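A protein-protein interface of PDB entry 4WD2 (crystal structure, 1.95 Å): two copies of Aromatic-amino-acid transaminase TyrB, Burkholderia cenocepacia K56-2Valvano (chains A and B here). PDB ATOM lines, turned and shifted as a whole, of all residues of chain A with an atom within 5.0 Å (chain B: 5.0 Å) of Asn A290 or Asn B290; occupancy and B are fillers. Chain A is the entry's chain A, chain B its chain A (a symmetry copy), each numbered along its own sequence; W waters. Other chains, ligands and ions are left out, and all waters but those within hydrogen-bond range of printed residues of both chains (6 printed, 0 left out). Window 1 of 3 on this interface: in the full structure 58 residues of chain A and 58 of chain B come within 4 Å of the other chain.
The backbone NH (N) of Ser A292 lies within hydrogen-bond range of the backbone carbonyl oxygen (O) of Val A287 (3.0 Å). The backbone carbonyl oxygen (O) of Ala B286 lies within hydrogen-bond range of the side-chain hydroxyl (OG) of Ser B289, at 2.7 Å. The side-chain carboxylate (OD1) of Asp A120 lies within salt-bridge range of the side-chain amino group (NZ) of Lys A116 (3.0 Å). OG of Ser A289 is in hydrogen-bond range of O of Ala A286 (2.7 Å). The backbone carbonyl oxygen (O) of Val B287 lies within hydrogen-bond range of the backbone NH (N) of Ser B292, 3.0 Å away. The side-chain amino group (NZ) of Lys B116 is in salt-bridge range of the side-chain carboxylate (OD1) of Asp B120 (3.0 Å).
Hydrophobic or aromatic side chains of chain B that line the printed part of chain A: Ile B144. Along chain A the printed residues that touch a printed residue of chain B span positions 112 to 292. Among the printed residues, 15 pairs touch across the chains.
Water W5 lies within hydrogen-bond range of O of Ile A144 (2.7 Å), O of Ser B289 (2.7 Å) and NZ of Lys A116 (2.8 Å). Water W4 lies within hydrogen-bond range of O of Ile B144 (2.7 Å), O of Ser A289 (2.7 Å) and NZ of Lys B116 (2.8 Å). Water W2 lies within hydrogen-bond range of the side-chain carboxylate of Asp B120 (2.7 Å), the side-chain amino group of Lys A116 (3.0 Å) and the side-chain hydroxyl of Ser B289 (3.1 Å). Water W1 lies within hydrogen-bond range of OD2 of Asp A120 (2.7 Å), NZ of Lys B116 (3.0 Å) and OG of Ser A289 (3.1 Å). Water W6 lies within hydrogen-bond range of the side-chain amide oxygen (OD1) of Asn B290 (3.0 Å) and the side-chain amide nitrogen (ND2) of Asn A290 (3.5 Å). Water W3 bridges OD1 of Asn A290 (3.0 Å) and ND2 of Asn B290 (3.5 Å).
O of Ser A112 touches O of Asn B290, 3.5 Å away. Ser A112 touches Tyr B291 (CB to C, 3.9 Å). O of Ser B289 touches CD of Lys A116 (3.4 Å). Lys A116 touches Asn B290. Ile A144 touches Arg B288. Arg A288 touches Ile B144 (O to CG1, 3.8 Å). Ser A289 touches Lys B116. Ser B112 touches Asn A290 (O to O, 3.5 Å). Asn A290 touches Lys B116 (O to CB, 3.2 Å). Ser B112 touches Tyr A291 (CB to C, 3.9 Å).
Ser A112 touches Asn B290, and with the chains exchanged Asn A290 touches Ser B112. Ser A112 touches Tyr B291, and with the chains exchanged Tyr A291 touches Ser B112. Ser A112 touches Ser B292, and with the chains exchanged Ser A292 touches Ser B112. Asn B290 touches its own counterpart, Asn A290. 12 positions are printed for both chains. Of the 15 pairs that touch across the chains among the printed residues, 15 have their exchanged pair printed and touching as well.
The side-chain hydroxyl (OG) of Ser A292 sits at hydrogen-bond distance from the side-chain hydroxyl (OG) of Ser B112 (2.7 Å). The side-chain amide oxygen (OD1) of Asn A290 is in hydrogen-bond range of the side-chain amide nitrogen (ND2) of Asn B290 (2.9 Å). The side-chain hydroxyl of Ser A112 is in hydrogen-bond range of the side-chain hydroxyl of Ser B292, 2.7 Å away.
Asn B290 touches just these residues of chain A: Ser A112, Lys A116 and Asn A290. Printed residues of chain A within 4 Å of Tyr B291: Ser A112 (3.9 Å). Of the printed residues of chain A, Arg B288 touches Ile A144 (3.8 Å). Of the printed residues of chain A, Ser B112 touches Asn A290 (3.5 Å), Tyr A291 (3.9 Å) and Ser A292 (2.7 Å). Of the printed residues of chain B, Ser A112 touches Asn B290, Tyr B291 and Ser B292. Printed residues of chain B within 4 Å of Ile A144: Arg B288 and Ser B289. Asp A120 touches none of the printed residues of chain B. Asp B120 touches none of the printed residues of chain A. The nearest residue of chain A that does not touch Asn B290 is Gly A113 (4.1 Å).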
ATOM      1  N   SER A 112     -25.774  19.793 -13.383  1.00  0.00           N
ATOM      2  CA  SER A 112     -24.911  18.615 -13.295  1.00  0.00           C
ATOM      3  C   SER A 112     -25.192  17.649 -14.428  1.00  0.00           C
ATOM      4  O   SER A 112     -24.270  17.156 -15.085  1.00  0.00           O
ATOM      5  CB  SER A 112     -25.104  17.880 -11.961  1.00  0.00           C
ATOM      6  OG  SER A 112     -24.796  18.696 -10.848  1.00  0.00           O
ATOM      7  N   GLY A 113     -26.476  17.359 -14.626  1.00  0.00           N
ATOM      8  CA  GLY A 113     -26.902  16.449 -15.668  1.00  0.00           C
ATOM      9  C   GLY A 113     -26.479  16.932 -17.039  1.00  0.00           C
ATOM     10  O   GLY A 113     -26.144  16.135 -17.911  1.00  0.00           O
ATOM     11  N   LYS A 116     -22.795  16.246 -17.430  1.00  0.00           N
ATOM     12  CA  LYS A 116     -22.606  14.816 -17.648  1.00  0.00           C
ATOM     13  C   LYS A 116     -22.928  14.407 -19.075  1.00  0.00           C
ATOM     14  O   LYS A 116     -22.128  13.729 -19.713  1.00  0.00           O
ATOM     15  CB  LYS A 116     -23.467  13.995 -16.683  1.00  0.00           C
ATOM     16  CG  LYS A 116     -23.400  12.486 -16.913  1.00  0.00           C
ATOM     17  CD  LYS A 116     -21.966  11.951 -16.811  1.00  0.00           C
ATOM     18  CE  LYS A 116     -21.927  10.423 -16.764  1.00  0.00           C
ATOM     19  NZ  LYS A 116     -20.536   9.931 -16.980  1.00  0.00           N
ATOM     20  N   ASP A 120     -20.209  13.007 -21.754  1.00  0.00           N
ATOM     21  CA  ASP A 120     -20.319  11.678 -22.358  1.00  0.00           C
ATOM     22  C   ASP A 120     -20.341  11.758 -23.898  1.00  0.00           C
ATOM     23  O   ASP A 120     -19.732  10.933 -24.581  1.00  0.00           O
ATOM     24  CB  ASP A 120     -21.571  10.951 -21.840  1.00  0.00           C
ATOM     25  CG  ASP A 120     -21.389  10.378 -20.426  1.00  0.00           C
ATOM     26  OD1 ASP A 120     -20.254  10.383 -19.906  1.00  0.00           O
ATOM     27  OD2 ASP A 120     -22.385   9.901 -19.843  1.00  0.00           O
ATOM     28  N   ILE A 144     -16.794  14.944 -12.312  1.00  0.00           N
ATOM     29  CA  ILE A 144     -17.646  14.564 -13.433  1.00  0.00           C
ATOM     30  C   ILE A 144     -16.819  14.249 -14.684  1.00  0.00           C
ATOM     31  O   ILE A 144     -16.993  13.199 -15.298  1.00  0.00           O
ATOM     32  CB  ILE A 144     -18.685  15.668 -13.749  1.00  0.00           C
ATOM     33  CG1 ILE A 144     -19.700  15.786 -12.609  1.00  0.00           C
ATOM     34  CG2 ILE A 144     -19.421  15.371 -15.044  1.00  0.00           C
ATOM     35  CD1 ILE A 144     -20.654  16.973 -12.752  1.00  0.00           C
ATOM     36  N   ALA A 286     -26.705   9.798 -25.495  1.00  0.00           N
ATOM     37  CA  ALA A 286     -26.057   9.831 -24.191  1.00  0.00           C
ATOM     38  C   ALA A 286     -27.087   9.654 -23.081  1.00  0.00           C
ATOM     39  O   ALA A 286     -26.858   8.927 -22.113  1.00  0.00           O
ATOM     40  CB  ALA A 286     -25.292  11.136 -24.004  1.00  0.00           C
ATOM     41  N   VAL A 287     -28.230  10.312 -23.241  1.00  0.00           N
ATOM     42  CA  VAL A 287     -29.345  10.167 -22.307  1.00  0.00           C
ATOM     43  C   VAL A 287     -29.859   8.722 -22.258  1.00  0.00           C
ATOM     44  O   VAL A 287     -30.119   8.182 -21.177  1.00  0.00           O
ATOM     45  CB  VAL A 287     -30.513  11.121 -22.680  1.00  0.00           C
ATOM     46  CG1 VAL A 287     -31.717  10.877 -21.783  1.00  0.00           C
ATOM     47  CG2 VAL A 287     -30.063  12.559 -22.574  1.00  0.00           C
ATOM     48  N   ARG A 288     -29.997   8.095 -23.426  1.00  0.00           N
ATOM     49  CA  ARG A 288     -30.464   6.709 -23.517  1.00  0.00           C
ATOM     50  C   ARG A 288     -29.546   5.740 -22.775  1.00  0.00           C
ATOM     51  O   ARG A 288     -29.994   4.721 -22.250  1.00  0.00           O
ATOM     52  CB  ARG A 288     -30.583   6.272 -24.986  1.00  0.00           C
ATOM     53  CG  ARG A 288     -31.092   4.848 -25.162  1.00  0.00           C
ATOM     54  CD  ARG A 288     -31.014   4.359 -26.610  1.00  0.00           C
ATOM     55  NE  ARG A 288     -31.383   2.947 -26.701  1.00  0.00           N
ATOM     56  CZ  ARG A 288     -31.081   2.144 -27.718  1.00  0.00           C
ATOM     57  NH1 ARG A 288     -30.398   2.610 -28.755  1.00  0.00           N
ATOM     58  NH2 ARG A 288     -31.465   0.871 -27.695  1.00  0.00           N
ATOM     59  N   SER A 289     -28.260   6.064 -22.739  1.00  0.00           N
ATOM     60  CA  SER A 289     -27.269   5.207 -22.106  1.00  0.00           C
ATOM     61  C   SER A 289     -27.213   5.470 -20.608  1.00  0.00           C
ATOM     62  O   SER A 289     -26.474   4.808 -19.877  1.00  0.00           O
ATOM     63  CB  SER A 289     -25.886   5.429 -22.735  1.00  0.00           C
ATOM     64  OG  SER A 289     -25.393   6.738 -22.479  1.00  0.00           O
ATOM     65  N   ASN A 290     -28.001   6.442 -20.159  1.00  0.00           N
ATOM     66  CA  ASN A 290     -27.928   6.931 -18.786  1.00  0.00           C
ATOM     67  C   ASN A 290     -29.240   6.709 -18.034  1.00  0.00           C
ATOM     68  O   ASN A 290     -29.371   5.738 -17.292  1.00  0.00           O
ATOM     69  CB  ASN A 290     -27.539   8.415 -18.786  1.00  0.00           C
ATOM     70  CG  ASN A 290     -27.124   8.919 -17.418  1.00  0.00           C
ATOM     71  OD1 ASN A 290     -27.496   8.348 -16.394  1.00  0.00           O
ATOM     72  ND2 ASN A 290     -26.356  10.008 -17.394  1.00  0.00           N
ATOM     73  N   TYR A 291     -30.215   7.596 -18.229  1.00  0.00           N
ATOM     74  CA  TYR A 291     -31.471   7.510 -17.487  1.00  0.00           C
ATOM     75  C   TYR A 291     -32.717   7.416 -18.383  1.00  0.00           C
ATOM     76  O   TYR A 291     -33.833   7.583 -17.896  1.00  0.00           O
ATOM     77  CB  TYR A 291     -31.598   8.711 -16.546  1.00  0.00           C
ATOM     78  CG  TYR A 291     -31.426  10.025 -17.255  1.00  0.00           C
ATOM     79  CD1 TYR A 291     -30.165  10.589 -17.413  1.00  0.00           C
ATOM     80  CD2 TYR A 291     -32.521  10.704 -17.772  1.00  0.00           C
ATOM     81  CE1 TYR A 291     -30.000  11.787 -18.075  1.00  0.00           C
ATOM     82  CE2 TYR A 291     -32.367  11.909 -18.431  1.00  0.00           C
ATOM     83  CZ  TYR A 291     -31.103  12.445 -18.578  1.00  0.00           C
ATOM     84  OH  TYR A 291     -30.938  13.644 -19.227  1.00  0.00           O
ATOM     85  N   SER A 292     -32.504   7.147 -19.674  1.00  0.00           N
ATOM     86  CA  SER A 292     -33.558   6.920 -20.689  1.00  0.00           C
ATOM     87  C   SER A 292     -34.320   8.173 -21.105  1.00  0.00           C
ATOM     88  O   SER A 292     -34.483   8.428 -22.298  1.00  0.00           O
ATOM     89  CB  SER A 292     -34.580   5.872 -20.223  1.00  0.00           C
ATOM     90  OG  SER A 292     -34.076   4.558 -20.343  1.00  0.00           O
ATOM     91  N   SER B 112     -33.976   2.424 -15.244  1.00  0.00           N
ATOM     92  CA  SER B 112     -32.846   2.744 -16.115  1.00  0.00           C
ATOM     93  C   SER B 112     -31.699   3.338 -15.321  1.00  0.00           C
ATOM     94  O   SER B 112     -30.542   2.937 -15.480  1.00  0.00           O
ATOM     95  CB  SER B 112     -33.250   3.736 -17.214  1.00  0.00           C
ATOM     96  OG  SER B 112     -34.275   3.229 -18.045  1.00  0.00           O
ATOM     97  N   GLY B 113     -32.031   4.323 -14.490  1.00  0.00           N
ATOM     98  CA  GLY B 113     -31.045   4.992 -13.668  1.00  0.00           C
ATOM     99  C   GLY B 113     -30.343   4.025 -12.738  1.00  0.00           C
ATOM    100  O   GLY B 113     -29.154   4.167 -12.464  1.00  0.00           O
ATOM    101  N   LYS B 116     -27.855   2.057 -14.769  1.00  0.00           N
ATOM    102  CA  LYS B 116     -26.715   2.914 -15.073  1.00  0.00           C
ATOM    103  C   LYS B 116     -25.776   3.057 -13.888  1.00  0.00           C
ATOM    104  O   LYS B 116     -24.571   2.873 -14.036  1.00  0.00           O
ATOM    105  CB  LYS B 116     -27.178   4.305 -15.518  1.00  0.00           C
ATOM    106  CG  LYS B 116     -26.041   5.296 -15.760  1.00  0.00           C
ATOM    107  CD  LYS B 116     -25.049   4.788 -16.815  1.00  0.00           C
ATOM    108  CE  LYS B 116     -24.076   5.880 -17.259  1.00  0.00           C
ATOM    109  NZ  LYS B 116     -22.946   5.287 -18.032  1.00  0.00           N
ATOM    110  N   ASP B 120     -21.962   1.648 -13.772  1.00  0.00           N
ATOM    111  CA  ASP B 120     -20.810   2.528 -13.577  1.00  0.00           C
ATOM    112  C   ASP B 120     -19.969   2.096 -12.359  1.00  0.00           C
ATOM    113  O   ASP B 120     -18.738   2.129 -12.399  1.00  0.00           O
ATOM    114  CB  ASP B 120     -21.264   3.989 -13.426  1.00  0.00           C
ATOM    115  CG  ASP B 120     -21.636   4.644 -14.766  1.00  0.00           C
ATOM    116  OD1 ASP B 120     -21.383   4.041 -15.831  1.00  0.00           O
ATOM    117  OD2 ASP B 120     -22.161   5.776 -14.751  1.00  0.00           O
ATOM    118  N   ILE B 144     -27.056   0.433 -22.555  1.00  0.00           N
ATOM    119  CA  ILE B 144     -26.576   0.973 -21.289  1.00  0.00           C
ATOM    120  C   ILE B 144     -25.233   0.354 -20.890  1.00  0.00           C
ATOM    121  O   ILE B 144     -24.283   1.071 -20.580  1.00  0.00           O
ATOM    122  CB  ILE B 144     -27.613   0.762 -20.159  1.00  0.00           C
ATOM    123  CG1 ILE B 144     -28.858   1.616 -20.411  1.00  0.00           C
ATOM    124  CG2 ILE B 144     -27.027   1.123 -18.804  1.00  0.00           C
ATOM    125  CD1 ILE B 144     -30.008   1.334 -19.442  1.00  0.00           C
ATOM    126  N   ALA B 286     -20.914   7.200  -7.893  1.00  0.00           N
ATOM    127  CA  ALA B 286     -21.380   7.089  -9.270  1.00  0.00           C
ATOM    128  C   ALA B 286     -22.426   8.159  -9.564  1.00  0.00           C
ATOM    129  O   ALA B 286     -22.413   8.782 -10.627  1.00  0.00           O
ATOM    130  CB  ALA B 286     -21.951   5.700  -9.532  1.00  0.00           C
ATOM    131  N   VAL B 287     -23.319   8.377  -8.605  1.00  0.00           N
ATOM    132  CA  VAL B 287     -24.324   9.434  -8.708  1.00  0.00           C
ATOM    133  C   VAL B 287     -23.677  10.822  -8.808  1.00  0.00           C
ATOM    134  O   VAL B 287     -24.092  11.652  -9.625  1.00  0.00           O
ATOM    135  CB  VAL B 287     -25.294   9.400  -7.495  1.00  0.00           C
ATOM    136  CG1 VAL B 287     -26.257  10.576  -7.542  1.00  0.00           C
ATOM    137  CG2 VAL B 287     -26.058   8.096  -7.478  1.00  0.00           C
ATOM    138  N   ARG B 288     -22.658  11.070  -7.986  1.00  0.00           N
ATOM    139  CA  ARG B 288     -21.944  12.350  -7.992  1.00  0.00           C
ATOM    140  C   ARG B 288     -21.303  12.648  -9.346  1.00  0.00           C
ATOM    141  O   ARG B 288     -21.178  13.805  -9.744  1.00  0.00           O
ATOM    142  CB  ARG B 288     -20.861  12.371  -6.901  1.00  0.00           C
ATOM    143  CG  ARG B 288     -20.094  13.684  -6.827  1.00  0.00           C
ATOM    144  CD  ARG B 288     -18.892  13.623  -5.880  1.00  0.00           C
ATOM    145  NE  ARG B 288     -18.115  14.859  -5.950  1.00  0.00           N
ATOM    146  CZ  ARG B 288     -16.853  14.990  -5.547  1.00  0.00           C
ATOM    147  NH1 ARG B 288     -16.208  13.952  -5.031  1.00  0.00           N
ATOM    148  NH2 ARG B 288     -16.238  16.163  -5.661  1.00  0.00           N
ATOM    149  N   SER B 289     -20.898  11.597 -10.046  1.00  0.00           N
ATOM    150  CA  SER B 289     -20.229  11.739 -11.330  1.00  0.00           C
ATOM    151  C   SER B 289     -21.249  11.890 -12.451  1.00  0.00           C
ATOM    152  O   SER B 289     -20.887  12.079 -13.612  1.00  0.00           O
ATOM    153  CB  SER B 289     -19.321  10.531 -11.600  1.00  0.00           C
ATOM    154  OG  SER B 289     -20.068   9.332 -11.756  1.00  0.00           O
ATOM    155  N   ASN B 290     -22.525  11.807 -12.088  1.00  0.00           N
ATOM    156  CA  ASN B 290     -23.608  11.753 -13.064  1.00  0.00           C
ATOM    157  C   ASN B 290     -24.554  12.946 -12.931  1.00  0.00           C
ATOM    158  O   ASN B 290     -24.430  13.920 -13.670  1.00  0.00           O
ATOM    159  CB  ASN B 290     -24.370  10.428 -12.919  1.00  0.00           C
ATOM    160  CG  ASN B 290     -25.291  10.142 -14.088  1.00  0.00           C
ATOM    161  OD1 ASN B 290     -25.707  11.053 -14.803  1.00  0.00           O
ATOM    162  ND2 ASN B 290     -25.626   8.868 -14.282  1.00  0.00           N
ATOM    163  N   TYR B 291     -25.491  12.881 -11.986  1.00  0.00           N
ATOM    164  CA  TYR B 291     -26.491  13.938 -11.842  1.00  0.00           C
ATOM    165  C   TYR B 291     -26.520  14.580 -10.446  1.00  0.00           C
ATOM    166  O   TYR B 291     -27.463  15.300 -10.124  1.00  0.00           O
ATOM    167  CB  TYR B 291     -27.876  13.388 -12.190  1.00  0.00           C
ATOM    168  CG  TYR B 291     -28.220  12.148 -11.413  1.00  0.00           C
ATOM    169  CD1 TYR B 291     -27.868  10.890 -11.888  1.00  0.00           C
ATOM    170  CD2 TYR B 291     -28.894  12.229 -10.202  1.00  0.00           C
ATOM    171  CE1 TYR B 291     -28.168   9.749 -11.174  1.00  0.00           C
ATOM    172  CE2 TYR B 291     -29.206  11.092  -9.482  1.00  0.00           C
ATOM    173  CZ  TYR B 291     -28.841   9.855  -9.974  1.00  0.00           C
ATOM    174  OH  TYR B 291     -29.149   8.718  -9.268  1.00  0.00           O
ATOM    175  N   SER B 292     -25.485  14.312  -9.645  1.00  0.00           N
ATOM    176  CA  SER B 292     -25.264  14.898  -8.302  1.00  0.00           C
ATOM    177  C   SER B 292     -26.201  14.376  -7.219  1.00  0.00           C
ATOM    178  O   SER B 292     -25.747  13.996  -6.141  1.00  0.00           O
ATOM    179  CB  SER B 292     -25.369  16.430  -8.326  1.00  0.00           C
ATOM    180  OG  SER B 292     -24.205  17.027  -8.861  1.00  0.00           O
HETATM  181  O   HOH W   1     -23.556   7.451 -20.084  1.00  0.00           O
HETATM  182  O   HOH W   2     -21.024   8.240 -14.498  1.00  0.00           O
HETATM  183  O   HOH W   3     -28.814   7.616 -13.789  1.00  0.00           O
HETATM  184  O   HOH W   4     -24.004   3.697 -20.025  1.00  0.00           O
HETATM  185  O   HOH W   5     -18.868  11.259 -15.226  1.00  0.00           O
HETATM  186  O   HOH W   6     -27.415  13.086 -16.221  1.00  0.00           O
